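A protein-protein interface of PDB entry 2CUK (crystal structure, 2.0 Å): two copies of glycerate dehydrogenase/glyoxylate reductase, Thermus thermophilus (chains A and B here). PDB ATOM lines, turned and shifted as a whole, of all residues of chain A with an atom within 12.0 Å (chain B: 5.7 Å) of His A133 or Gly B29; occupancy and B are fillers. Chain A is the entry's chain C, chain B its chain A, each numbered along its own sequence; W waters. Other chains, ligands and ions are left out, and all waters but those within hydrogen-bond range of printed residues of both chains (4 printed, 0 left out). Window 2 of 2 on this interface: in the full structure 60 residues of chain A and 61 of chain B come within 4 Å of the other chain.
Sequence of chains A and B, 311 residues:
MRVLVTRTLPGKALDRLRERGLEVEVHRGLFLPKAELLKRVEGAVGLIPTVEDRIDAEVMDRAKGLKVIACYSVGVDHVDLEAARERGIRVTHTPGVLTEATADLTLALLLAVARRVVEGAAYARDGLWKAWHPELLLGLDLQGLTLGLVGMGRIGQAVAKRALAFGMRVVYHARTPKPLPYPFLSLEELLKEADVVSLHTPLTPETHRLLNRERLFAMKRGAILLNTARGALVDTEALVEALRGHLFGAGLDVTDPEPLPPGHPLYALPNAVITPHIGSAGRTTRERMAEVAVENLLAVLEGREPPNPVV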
ATOM      1  N   ARG A 115      -4.343  27.372  17.854  1.00  0.00           N
ATOM      2  CA  ARG A 115      -4.219  26.714  19.148  1.00  0.00           C
ATOM      3  C   ARG A 115      -5.289  25.658  19.448  1.00  0.00           C
ATOM      4  O   ARG A 115      -5.414  25.197  20.584  1.00  0.00           O
ATOM      5  CB  ARG A 115      -4.164  27.765  20.263  1.00  0.00           C
ATOM      6  CG  ARG A 115      -3.004  28.755  20.109  1.00  0.00           C
ATOM      7  CD  ARG A 115      -1.656  28.035  20.007  1.00  0.00           C
ATOM      8  NE  ARG A 115      -1.424  27.190  21.176  1.00  0.00           N
ATOM      9  CZ  ARG A 115      -1.019  27.643  22.358  1.00  0.00           C
ATOM     10  NH1 ARG A 115      -0.783  28.938  22.535  1.00  0.00           N
ATOM     11  NH2 ARG A 115      -0.877  26.803  23.374  1.00  0.00           N
ATOM     12  N   ARG A 116      -6.051  25.275  18.425  1.00  0.00           N
ATOM     13  CA  ARG A 116      -7.067  24.230  18.565  1.00  0.00           C
ATOM     14  C   ARG A 116      -7.949  24.407  19.803  1.00  0.00           C
ATOM     15  O   ARG A 116      -8.149  23.471  20.581  1.00  0.00           O
ATOM     16  CB  ARG A 116      -6.358  22.870  18.607  1.00  0.00           C
ATOM     17  CG  ARG A 116      -5.399  22.669  17.424  1.00  0.00           C
ATOM     18  CD  ARG A 116      -4.484  21.455  17.587  1.00  0.00           C
ATOM     19  NE  ARG A 116      -5.219  20.193  17.576  1.00  0.00           N
ATOM     20  CZ  ARG A 116      -4.652  18.993  17.665  1.00  0.00           C
ATOM     21  NH1 ARG A 116      -3.332  18.880  17.773  1.00  0.00           N
ATOM     22  NH2 ARG A 116      -5.405  17.899  17.646  1.00  0.00           N
ATOM     23  N   TYR A 123     -12.810  18.341  23.562  1.00  0.00           N
ATOM     24  CA  TYR A 123     -12.024  17.282  24.191  1.00  0.00           C
ATOM     25  C   TYR A 123     -12.348  17.194  25.684  1.00  0.00           C
ATOM     26  O   TYR A 123     -12.567  16.107  26.222  1.00  0.00           O
ATOM     27  CB  TYR A 123     -10.532  17.580  23.989  1.00  0.00           C
ATOM     28  CG  TYR A 123      -9.585  16.545  24.548  1.00  0.00           C
ATOM     29  CD1 TYR A 123      -9.297  15.378  23.840  1.00  0.00           C
ATOM     30  CD2 TYR A 123      -8.967  16.735  25.784  1.00  0.00           C
ATOM     31  CE1 TYR A 123      -8.410  14.424  24.350  1.00  0.00           C
ATOM     32  CE2 TYR A 123      -8.082  15.788  26.304  1.00  0.00           C
ATOM     33  CZ  TYR A 123      -7.810  14.637  25.581  1.00  0.00           C
ATOM     34  OH  TYR A 123      -6.950  13.696  26.096  1.00  0.00           O
ATOM     35  N   LEU A 128     -12.651  13.302  27.559  1.00  0.00           N
ATOM     36  CA  LEU A 128     -11.389  12.669  27.185  1.00  0.00           C
ATOM     37  C   LEU A 128     -10.207  13.245  27.967  1.00  0.00           C
ATOM     38  O   LEU A 128      -9.109  12.690  27.945  1.00  0.00           O
ATOM     39  CB  LEU A 128     -11.138  12.831  25.685  1.00  0.00           C
ATOM     40  CG  LEU A 128     -12.206  12.225  24.772  1.00  0.00           C
ATOM     41  CD1 LEU A 128     -11.836  12.473  23.315  1.00  0.00           C
ATOM     42  CD2 LEU A 128     -12.331  10.730  25.056  1.00  0.00           C
ATOM     43  N   TRP A 129     -10.442  14.352  28.666  1.00  0.00           N
ATOM     44  CA  TRP A 129      -9.394  15.007  29.443  1.00  0.00           C
ATOM     45  C   TRP A 129      -9.102  14.234  30.726  1.00  0.00           C
ATOM     46  O   TRP A 129      -9.860  14.301  31.698  1.00  0.00           O
ATOM     47  CB  TRP A 129      -9.819  16.443  29.761  1.00  0.00           C
ATOM     48  CG  TRP A 129      -8.804  17.263  30.506  1.00  0.00           C
ATOM     49  CD1 TRP A 129      -7.459  17.030  30.607  1.00  0.00           C
ATOM     50  CD2 TRP A 129      -9.054  18.486  31.212  1.00  0.00           C
ATOM     51  NE1 TRP A 129      -6.857  18.035  31.335  1.00  0.00           N
ATOM     52  CE2 TRP A 129      -7.813  18.941  31.716  1.00  0.00           C
ATOM     53  CE3 TRP A 129     -10.208  19.242  31.466  1.00  0.00           C
ATOM     54  CZ2 TRP A 129      -7.692  20.120  32.462  1.00  0.00           C
ATOM     55  CZ3 TRP A 129     -10.087  20.422  32.210  1.00  0.00           C
ATOM     56  CH2 TRP A 129      -8.838  20.845  32.697  1.00  0.00           C
ATOM     57  N   LYS A 130      -7.993  13.502  30.725  1.00  0.00           N
ATOM     58  CA  LYS A 130      -7.618  12.702  31.880  1.00  0.00           C
ATOM     59  C   LYS A 130      -6.274  13.094  32.485  1.00  0.00           C
ATOM     60  O   LYS A 130      -5.964  12.711  33.606  1.00  0.00           O
ATOM     61  CB  LYS A 130      -7.613  11.225  31.487  1.00  0.00           C
ATOM     62  CG  LYS A 130      -8.939  10.786  30.887  1.00  0.00           C
ATOM     63  CD  LYS A 130      -8.940   9.322  30.500  1.00  0.00           C
ATOM     64  CE  LYS A 130     -10.252   8.951  29.824  1.00  0.00           C
ATOM     65  NZ  LYS A 130     -11.420   9.346  30.662  1.00  0.00           N
ATOM     66  N   ALA A 131      -5.477  13.858  31.745  1.00  0.00           N
ATOM     67  CA  ALA A 131      -4.179  14.292  32.250  1.00  0.00           C
ATOM     68  C   ALA A 131      -3.493  15.286  31.327  1.00  0.00           C
ATOM     69  O   ALA A 131      -3.899  15.479  30.179  1.00  0.00           O
ATOM     70  CB  ALA A 131      -3.269  13.081  32.456  1.00  0.00           C
ATOM     71  N   TRP A 132      -2.453  15.927  31.851  1.00  0.00           N
ATOM     72  CA  TRP A 132      -1.660  16.877  31.080  1.00  0.00           C
ATOM     73  C   TRP A 132      -0.605  16.013  30.391  1.00  0.00           C
ATOM     74  O   TRP A 132      -0.096  15.070  30.995  1.00  0.00           O
ATOM     75  CB  TRP A 132      -0.962  17.869  32.013  1.00  0.00           C
ATOM     76  CG  TRP A 132      -0.154  18.903  31.293  1.00  0.00           C
ATOM     77  CD1 TRP A 132      -0.577  20.131  30.878  1.00  0.00           C
ATOM     78  CD2 TRP A 132       1.211  18.785  30.868  1.00  0.00           C
ATOM     79  NE1 TRP A 132       0.437  20.787  30.222  1.00  0.00           N
ATOM     80  CE2 TRP A 132       1.545  19.984  30.202  1.00  0.00           C
ATOM     81  CE3 TRP A 132       2.182  17.782  30.986  1.00  0.00           C
ATOM     82  CZ2 TRP A 132       2.812  20.211  29.653  1.00  0.00           C
ATOM     83  CZ3 TRP A 132       3.446  18.007  30.440  1.00  0.00           C
ATOM     84  CH2 TRP A 132       3.747  19.213  29.782  1.00  0.00           C
ATOM     85  N   HIS A 133      -0.280  16.316  29.138  1.00  0.00           N
ATOM     86  CA  HIS A 133       0.732  15.536  28.424  1.00  0.00           C
ATOM     87  C   HIS A 133       1.514  16.437  27.468  1.00  0.00           C
ATOM     88  O   HIS A 133       0.948  17.330  26.847  1.00  0.00           O
ATOM     89  CB  HIS A 133       0.078  14.390  27.637  1.00  0.00           C
ATOM     90  CG  HIS A 133       1.058  13.390  27.107  1.00  0.00           C
ATOM     91  ND1 HIS A 133       1.692  13.539  25.890  1.00  0.00           N
ATOM     92  CD2 HIS A 133       1.473  12.201  27.602  1.00  0.00           C
ATOM     93  CE1 HIS A 133       2.454  12.484  25.661  1.00  0.00           C
ATOM     94  NE2 HIS A 133       2.338  11.656  26.684  1.00  0.00           N
ATOM     95  N   PRO A 134       2.833  16.213  27.344  1.00  0.00           N
ATOM     96  CA  PRO A 134       3.680  17.018  26.458  1.00  0.00           C
ATOM     97  C   PRO A 134       3.203  17.108  25.010  1.00  0.00           C
ATOM     98  O   PRO A 134       3.443  18.107  24.341  1.00  0.00           O
ATOM     99  CB  PRO A 134       5.045  16.334  26.569  1.00  0.00           C
ATOM    100  CG  PRO A 134       5.035  15.791  27.958  1.00  0.00           C
ATOM    101  CD  PRO A 134       3.641  15.214  28.068  1.00  0.00           C
ATOM    102  N   GLU A 135       2.517  16.078  24.526  1.00  0.00           N
ATOM    103  CA  GLU A 135       2.057  16.073  23.140  1.00  0.00           C
ATOM    104  C   GLU A 135       0.542  16.181  22.944  1.00  0.00           C
ATOM    105  O   GLU A 135       0.035  15.888  21.867  1.00  0.00           O
ATOM    106  CB  GLU A 135       2.563  14.812  22.440  1.00  0.00           C
ATOM    107  CG  GLU A 135       4.041  14.540  22.671  1.00  0.00           C
ATOM    108  CD  GLU A 135       4.516  13.285  21.967  1.00  0.00           C
ATOM    109  OE1 GLU A 135       5.108  13.401  20.872  1.00  0.00           O
ATOM    110  OE2 GLU A 135       4.286  12.183  22.504  1.00  0.00           O
ATOM    111  N   LEU A 136      -0.180  16.608  23.968  1.00  0.00           N
ATOM    112  CA  LEU A 136      -1.628  16.735  23.851  1.00  0.00           C
ATOM    113  C   LEU A 136      -2.042  18.042  23.169  1.00  0.00           C
ATOM    114  O   LEU A 136      -1.622  19.122  23.578  1.00  0.00           O
ATOM    115  CB  LEU A 136      -2.274  16.664  25.233  1.00  0.00           C
ATOM    116  CG  LEU A 136      -3.804  16.738  25.260  1.00  0.00           C
ATOM    117  CD1 LEU A 136      -4.385  15.494  24.603  1.00  0.00           C
ATOM    118  CD2 LEU A 136      -4.293  16.853  26.694  1.00  0.00           C
ATOM    119  N   LEU A 137      -2.864  17.924  22.125  1.00  0.00           N
ATOM    120  CA  LEU A 137      -3.391  19.071  21.382  1.00  0.00           C
ATOM    121  C   LEU A 137      -2.372  20.144  20.984  1.00  0.00           C
ATOM    122  O   LEU A 137      -2.598  21.338  21.197  1.00  0.00           O
ATOM    123  CB  LEU A 137      -4.520  19.707  22.198  1.00  0.00           C
ATOM    124  CG  LEU A 137      -5.766  18.829  22.353  1.00  0.00           C
ATOM    125  CD1 LEU A 137      -6.568  19.236  23.592  1.00  0.00           C
ATOM    126  CD2 LEU A 137      -6.607  18.945  21.095  1.00  0.00           C
ATOM    127  N   LEU A 138      -1.258  19.716  20.395  1.00  0.00           N
ATOM    128  CA  LEU A 138      -0.209  20.640  19.968  1.00  0.00           C
ATOM    129  C   LEU A 138      -0.673  21.511  18.800  1.00  0.00           C
ATOM    130  O   LEU A 138      -1.257  21.016  17.837  1.00  0.00           O
ATOM    131  CB  LEU A 138       1.046  19.856  19.565  1.00  0.00           C
ATOM    132  CG  LEU A 138       1.742  19.061  20.676  1.00  0.00           C
ATOM    133  CD1 LEU A 138       2.927  18.284  20.108  1.00  0.00           C
ATOM    134  CD2 LEU A 138       2.206  20.022  21.769  1.00  0.00           C
ATOM    135  N   GLY A 139      -0.416  22.811  18.891  1.00  0.00           N
ATOM    136  CA  GLY A 139      -0.825  23.713  17.831  1.00  0.00           C
ATOM    137  C   GLY A 139       0.342  24.460  17.216  1.00  0.00           C
ATOM    138  O   GLY A 139       1.484  24.006  17.300  1.00  0.00           O
ATOM    139  N   THR B   6       9.705  10.701  31.967  1.00  0.00           N
ATOM    140  CA  THR B   6       8.377  10.235  32.353  1.00  0.00           C
ATOM    141  C   THR B   6       7.268  10.285  31.306  1.00  0.00           C
ATOM    142  O   THR B   6       6.216   9.677  31.499  1.00  0.00           O
ATOM    143  CB  THR B   6       7.891  10.976  33.606  1.00  0.00           C
ATOM    144  OG1 THR B   6       7.761  12.374  33.317  1.00  0.00           O
ATOM    145  CG2 THR B   6       8.890  10.784  34.750  1.00  0.00           C
ATOM    146  N   ARG B   7       7.492  11.001  30.209  1.00  0.00           N
ATOM    147  CA  ARG B   7       6.490  11.099  29.146  1.00  0.00           C
ATOM    148  C   ARG B   7       7.161  11.280  27.791  1.00  0.00           C
ATOM    149  O   ARG B   7       8.296  11.745  27.712  1.00  0.00           O
ATOM    150  CB  ARG B   7       5.556  12.291  29.388  1.00  0.00           C
ATOM    151  CG  ARG B   7       4.725  12.224  30.653  1.00  0.00           C
ATOM    152  CD  ARG B   7       3.684  11.112  30.609  1.00  0.00           C
ATOM    153  NE  ARG B   7       2.790  11.195  31.762  1.00  0.00           N
ATOM    154  CZ  ARG B   7       3.184  11.066  33.026  1.00  0.00           C
ATOM    155  NH1 ARG B   7       4.462  10.836  33.306  1.00  0.00           N
ATOM    156  NH2 ARG B   7       2.307  11.193  34.013  1.00  0.00           N
ATOM    157  N   THR B   8       6.456  10.915  26.723  1.00  0.00           N
ATOM    158  CA  THR B   8       6.998  11.083  25.382  1.00  0.00           C
ATOM    159  C   THR B   8       7.001  12.577  25.070  1.00  0.00           C
ATOM    160  O   THR B   8       6.074  13.298  25.445  1.00  0.00           O
ATOM    161  CB  THR B   8       6.153  10.343  24.337  1.00  0.00           C
ATOM    162  OG1 THR B   8       4.775  10.699  24.499  1.00  0.00           O
ATOM    163  CG2 THR B   8       6.304   8.838  24.500  1.00  0.00           C
ATOM    164  N   HIS B  27       8.888   6.836  28.769  1.00  0.00           N
ATOM    165  CA  HIS B  27       7.652   6.164  29.148  1.00  0.00           C
ATOM    166  C   HIS B  27       6.475   6.604  28.273  1.00  0.00           C
ATOM    167  O   HIS B  27       6.171   7.783  28.135  1.00  0.00           O
ATOM    168  CB  HIS B  27       7.373   6.528  30.607  1.00  0.00           C
ATOM    169  CG  HIS B  27       6.076   5.907  31.047  1.00  0.00           C
ATOM    170  ND1 HIS B  27       5.940   4.588  31.317  1.00  0.00           N
ATOM    171  CD2 HIS B  27       4.841   6.533  31.243  1.00  0.00           C
ATOM    172  CE1 HIS B  27       4.651   4.420  31.666  1.00  0.00           C
ATOM    173  NE2 HIS B  27       3.969   5.569  31.630  1.00  0.00           N
ATOM    174  N   ARG B  28       5.826   5.607  27.638  1.00  0.00           N
ATOM    175  CA  ARG B  28       4.695   5.921  26.770  1.00  0.00           C
ATOM    176  C   ARG B  28       3.364   5.872  27.528  1.00  0.00           C
ATOM    177  O   ARG B  28       3.190   5.135  28.488  1.00  0.00           O
ATOM    178  CB  ARG B  28       4.667   4.896  25.631  1.00  0.00           C
ATOM    179  CG  ARG B  28       5.970   4.853  24.835  1.00  0.00           C
ATOM    180  CD  ARG B  28       5.940   3.755  23.766  1.00  0.00           C
ATOM    181  NE  ARG B  28       4.804   3.950  22.857  1.00  0.00           N
ATOM    182  CZ  ARG B  28       4.232   2.848  22.334  1.00  0.00           C
ATOM    183  NH1 ARG B  28       4.686   1.648  22.649  1.00  0.00           N
ATOM    184  NH2 ARG B  28       3.208   2.977  21.486  1.00  0.00           N
ATOM    185  N   GLY B  29       2.418   6.726  27.093  1.00  0.00           N
ATOM    186  CA  GLY B  29       1.082   6.681  27.683  1.00  0.00           C
ATOM    187  C   GLY B  29       0.745   7.959  28.452  1.00  0.00           C
ATOM    188  O   GLY B  29       1.571   8.839  28.641  1.00  0.00           O
ATOM    189  N   LEU B  30      -0.506   8.010  28.896  1.00  0.00           N
ATOM    190  CA  LEU B  30      -1.040   9.151  29.620  1.00  0.00           C
ATOM    191  C   LEU B  30      -0.816   9.080  31.131  1.00  0.00           C
ATOM    192  O   LEU B  30      -0.877  10.102  31.816  1.00  0.00           O
ATOM    193  CB  LEU B  30      -2.537   9.263  29.331  1.00  0.00           C
ATOM    194  CG  LEU B  30      -3.101  10.627  28.936  1.00  0.00           C
ATOM    195  CD1 LEU B  30      -2.340  11.190  27.748  1.00  0.00           C
ATOM    196  CD2 LEU B  30      -4.577  10.465  28.603  1.00  0.00           C
ATOM    197  N   PHE B  31      -0.555   7.882  31.648  1.00  0.00           N
ATOM    198  CA  PHE B  31      -0.350   7.703  33.084  1.00  0.00           C
ATOM    199  C   PHE B  31       0.949   6.990  33.451  1.00  0.00           C
ATOM    200  O   PHE B  31       1.468   6.178  32.683  1.00  0.00           O
ATOM    201  CB  PHE B  31      -1.517   6.913  33.684  1.00  0.00           C
ATOM    202  CG  PHE B  31      -2.854   7.575  33.516  1.00  0.00           C
ATOM    203  CD1 PHE B  31      -3.206   8.674  34.294  1.00  0.00           C
ATOM    204  CD2 PHE B  31      -3.759   7.106  32.568  1.00  0.00           C
ATOM    205  CE1 PHE B  31      -4.444   9.300  34.133  1.00  0.00           C
ATOM    206  CE2 PHE B  31      -4.998   7.721  32.396  1.00  0.00           C
ATOM    207  CZ  PHE B  31      -5.341   8.822  33.181  1.00  0.00           C
ATOM    208  N   GLU B  52       2.889  16.157  36.226  1.00  0.00           N
ATOM    209  CA  GLU B  52       2.045  15.038  36.651  1.00  0.00           C
ATOM    210  C   GLU B  52       2.802  13.987  37.465  1.00  0.00           C
ATOM    211  O   GLU B  52       2.208  13.007  37.918  1.00  0.00           O
ATOM    212  CB  GLU B  52       1.419  14.354  35.429  1.00  0.00           C
ATOM    213  CG  GLU B  52       0.506  15.240  34.592  1.00  0.00           C
ATOM    214  CD  GLU B  52      -0.864  15.436  35.213  1.00  0.00           C
ATOM    215  OE1 GLU B  52      -0.935  15.770  36.415  1.00  0.00           O
ATOM    216  OE2 GLU B  52      -1.872  15.264  34.494  1.00  0.00           O
ATOM    217  N   ARG B 286       6.748  23.438  22.930  1.00  0.00           N
ATOM    218  CA  ARG B 286       6.966  22.145  23.572  1.00  0.00           C
ATOM    219  C   ARG B 286       8.293  21.493  23.148  1.00  0.00           C
ATOM    220  O   ARG B 286       8.932  20.797  23.944  1.00  0.00           O
ATOM    221  CB  ARG B 286       5.782  21.207  23.299  1.00  0.00           C
ATOM    222  CG  ARG B 286       4.489  21.591  24.054  1.00  0.00           C
ATOM    223  CD  ARG B 286       4.611  21.364  25.560  1.00  0.00           C
ATOM    224  NE  ARG B 286       3.451  21.864  26.309  1.00  0.00           N
ATOM    225  CZ  ARG B 286       2.244  21.301  26.307  1.00  0.00           C
ATOM    226  NH1 ARG B 286       2.016  20.202  25.598  1.00  0.00           N
ATOM    227  NH2 ARG B 286       1.257  21.842  27.013  1.00  0.00           N
HETATM  228  O   HOH W   1      -0.807  19.994  26.106  1.00  0.00           O
HETATM  229  O   HOH W   2       4.143   9.349  27.487  1.00  0.00           O
HETATM  230  O   HOH W   3       0.404  12.392  30.948  1.00  0.00           O
HETATM  231  O   HOH W   4      -0.064  23.572  29.015  1.00  0.00           O
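The backbone carbonyl oxygen (O) of His B27 lies within hydrogen-bond range of the backbone NH (N) of Thr B8.
NE2 of His B27 sits at hydrogen-bond distance from O of Phe B31, 2.8 Å away.
O of Leu A138 lies within hydrogen-bond range of NH1 of Arg A116 (3.0 Å).
N of Glu A135 sits at hydrogen-bond distance from ND1 of His A133.
Hydrophobic or aromatic side chains of chain A within 4 Å of the printed part of chain B: Ala A131, Trp A132, His A133, Pro A134 and Leu A138.
Hydrophobic or aromatic side chains of chain B within 4 Å of the printed part of chain A: Leu B30 and Phe B31.
Along chain B the printed residues that touch a printed residue of chain A span positions 7 to 286.
Among the printed residues, 15 pairs touch across the chains.
Water W2 lies within hydrogen-bond range of O of His B27 (2.6 Å), O of Gly B29 (2.9 Å), N of Thr B8 (2.9 Å) and NE2 of His A133 (3.0 Å).
Water W3 lies within hydrogen-bond range of O of Trp A132, O of Leu B30 and NE of Arg B7.
Water W1 lies within hydrogen-bond range of O of Leu A136 (2.8 Å), NH1 of Arg B286 (2.9 Å) and O of His A133 (3.3 Å).
Water W4 bridges NH2 of Arg B286 (3.0 Å) and NE1 of Trp A132 (3.1 Å).
No position is printed for both chains.
Of the 15 pairs that touch across the chains among the printed residues, none has its exchanged pair printed and touching as well.
His A133 touches just these residues of chain B: Arg B7 (3.9 Å), Thr B8 (3.2 Å), Gly B29 (3.5 Å), Leu B30 (3.9 Å) and Arg B286 (3.3 Å).
Arg B7 touches two residues of chain A.
Of chain A, only His A133, Pro A134 and Glu A135 come within 4 Å of Thr B8.
Leu B30 touches just these residues of chain A: Ala A131 and His A133.
Phe B31 touches one residue of chain A.
Printed residues of chain B within 4 Å of Glu A135: Thr B8 (2.5 Å).
Of the printed residues of chain A, Arg B286 touches Trp A132 (3.5 Å), His A133 (3.3 Å), Pro A134 (2.8 Å) and Leu A138 (3.6 Å).
Printed residues of chain B within 4 Å of Lys A130: Phe B31.
Printed residues of chain B within 4 Å of Pro A134: Arg B7, Thr B8 and Arg B286.
Of the printed residues of chain B, Ala A131 touches Leu B30 (3.9 Å) and Glu B52 (3.3 Å).
The nearest printed residue of chain B that does not touch His A133 is Glu B52 (5.6 Å).
The nearest printed residue of chain A that does not touch Glu B52 is Lys A130 (4.9 Å).
A ring nitrogen (NE2) of His A133 lies close to the side-chain hydroxyl (OG1) of Thr B8 (3.4 Å).
The side-chain hydroxyl (OG1) of Thr B8 lies within hydrogen-bond range of the side-chain carboxylate (OE2) of Glu A135, 2.5 Å away.
The backbone NH of Trp A132 sits at hydrogen-bond distance from the side-chain carboxylate of Glu B52, 2.8 Å away.
O of His A133 sits at hydrogen-bond distance from NH1 of Arg B286.
NH1 of Arg B286 sits at hydrogen-bond distance from O of Pro A134 (2.8 Å).
The indole nitrogen (NE1) of Trp A132 lies close to the guanidinium group (NH2) of Arg B286 (3.5 Å).
Lys A130 touches Phe B31 (CB to CZ, 3.7 Å).
Ala A131 touches Leu B30.
Glu B52 touches Ala A131 (OE2 to CB, 3.3 Å).
CD2 of His A133 touches CD of Arg B7, at 3.9 Å.
Gly B29 touches His A133.
Leu B30 touches His A133 (CD1 to CD2, 3.9 Å).
Pro A134 touches Arg B7 (CD to CB, 3.7 Å).
Thr B8 touches Pro A134 (O to CB, 3.4 Å).
Leu A138 touches Arg B286.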
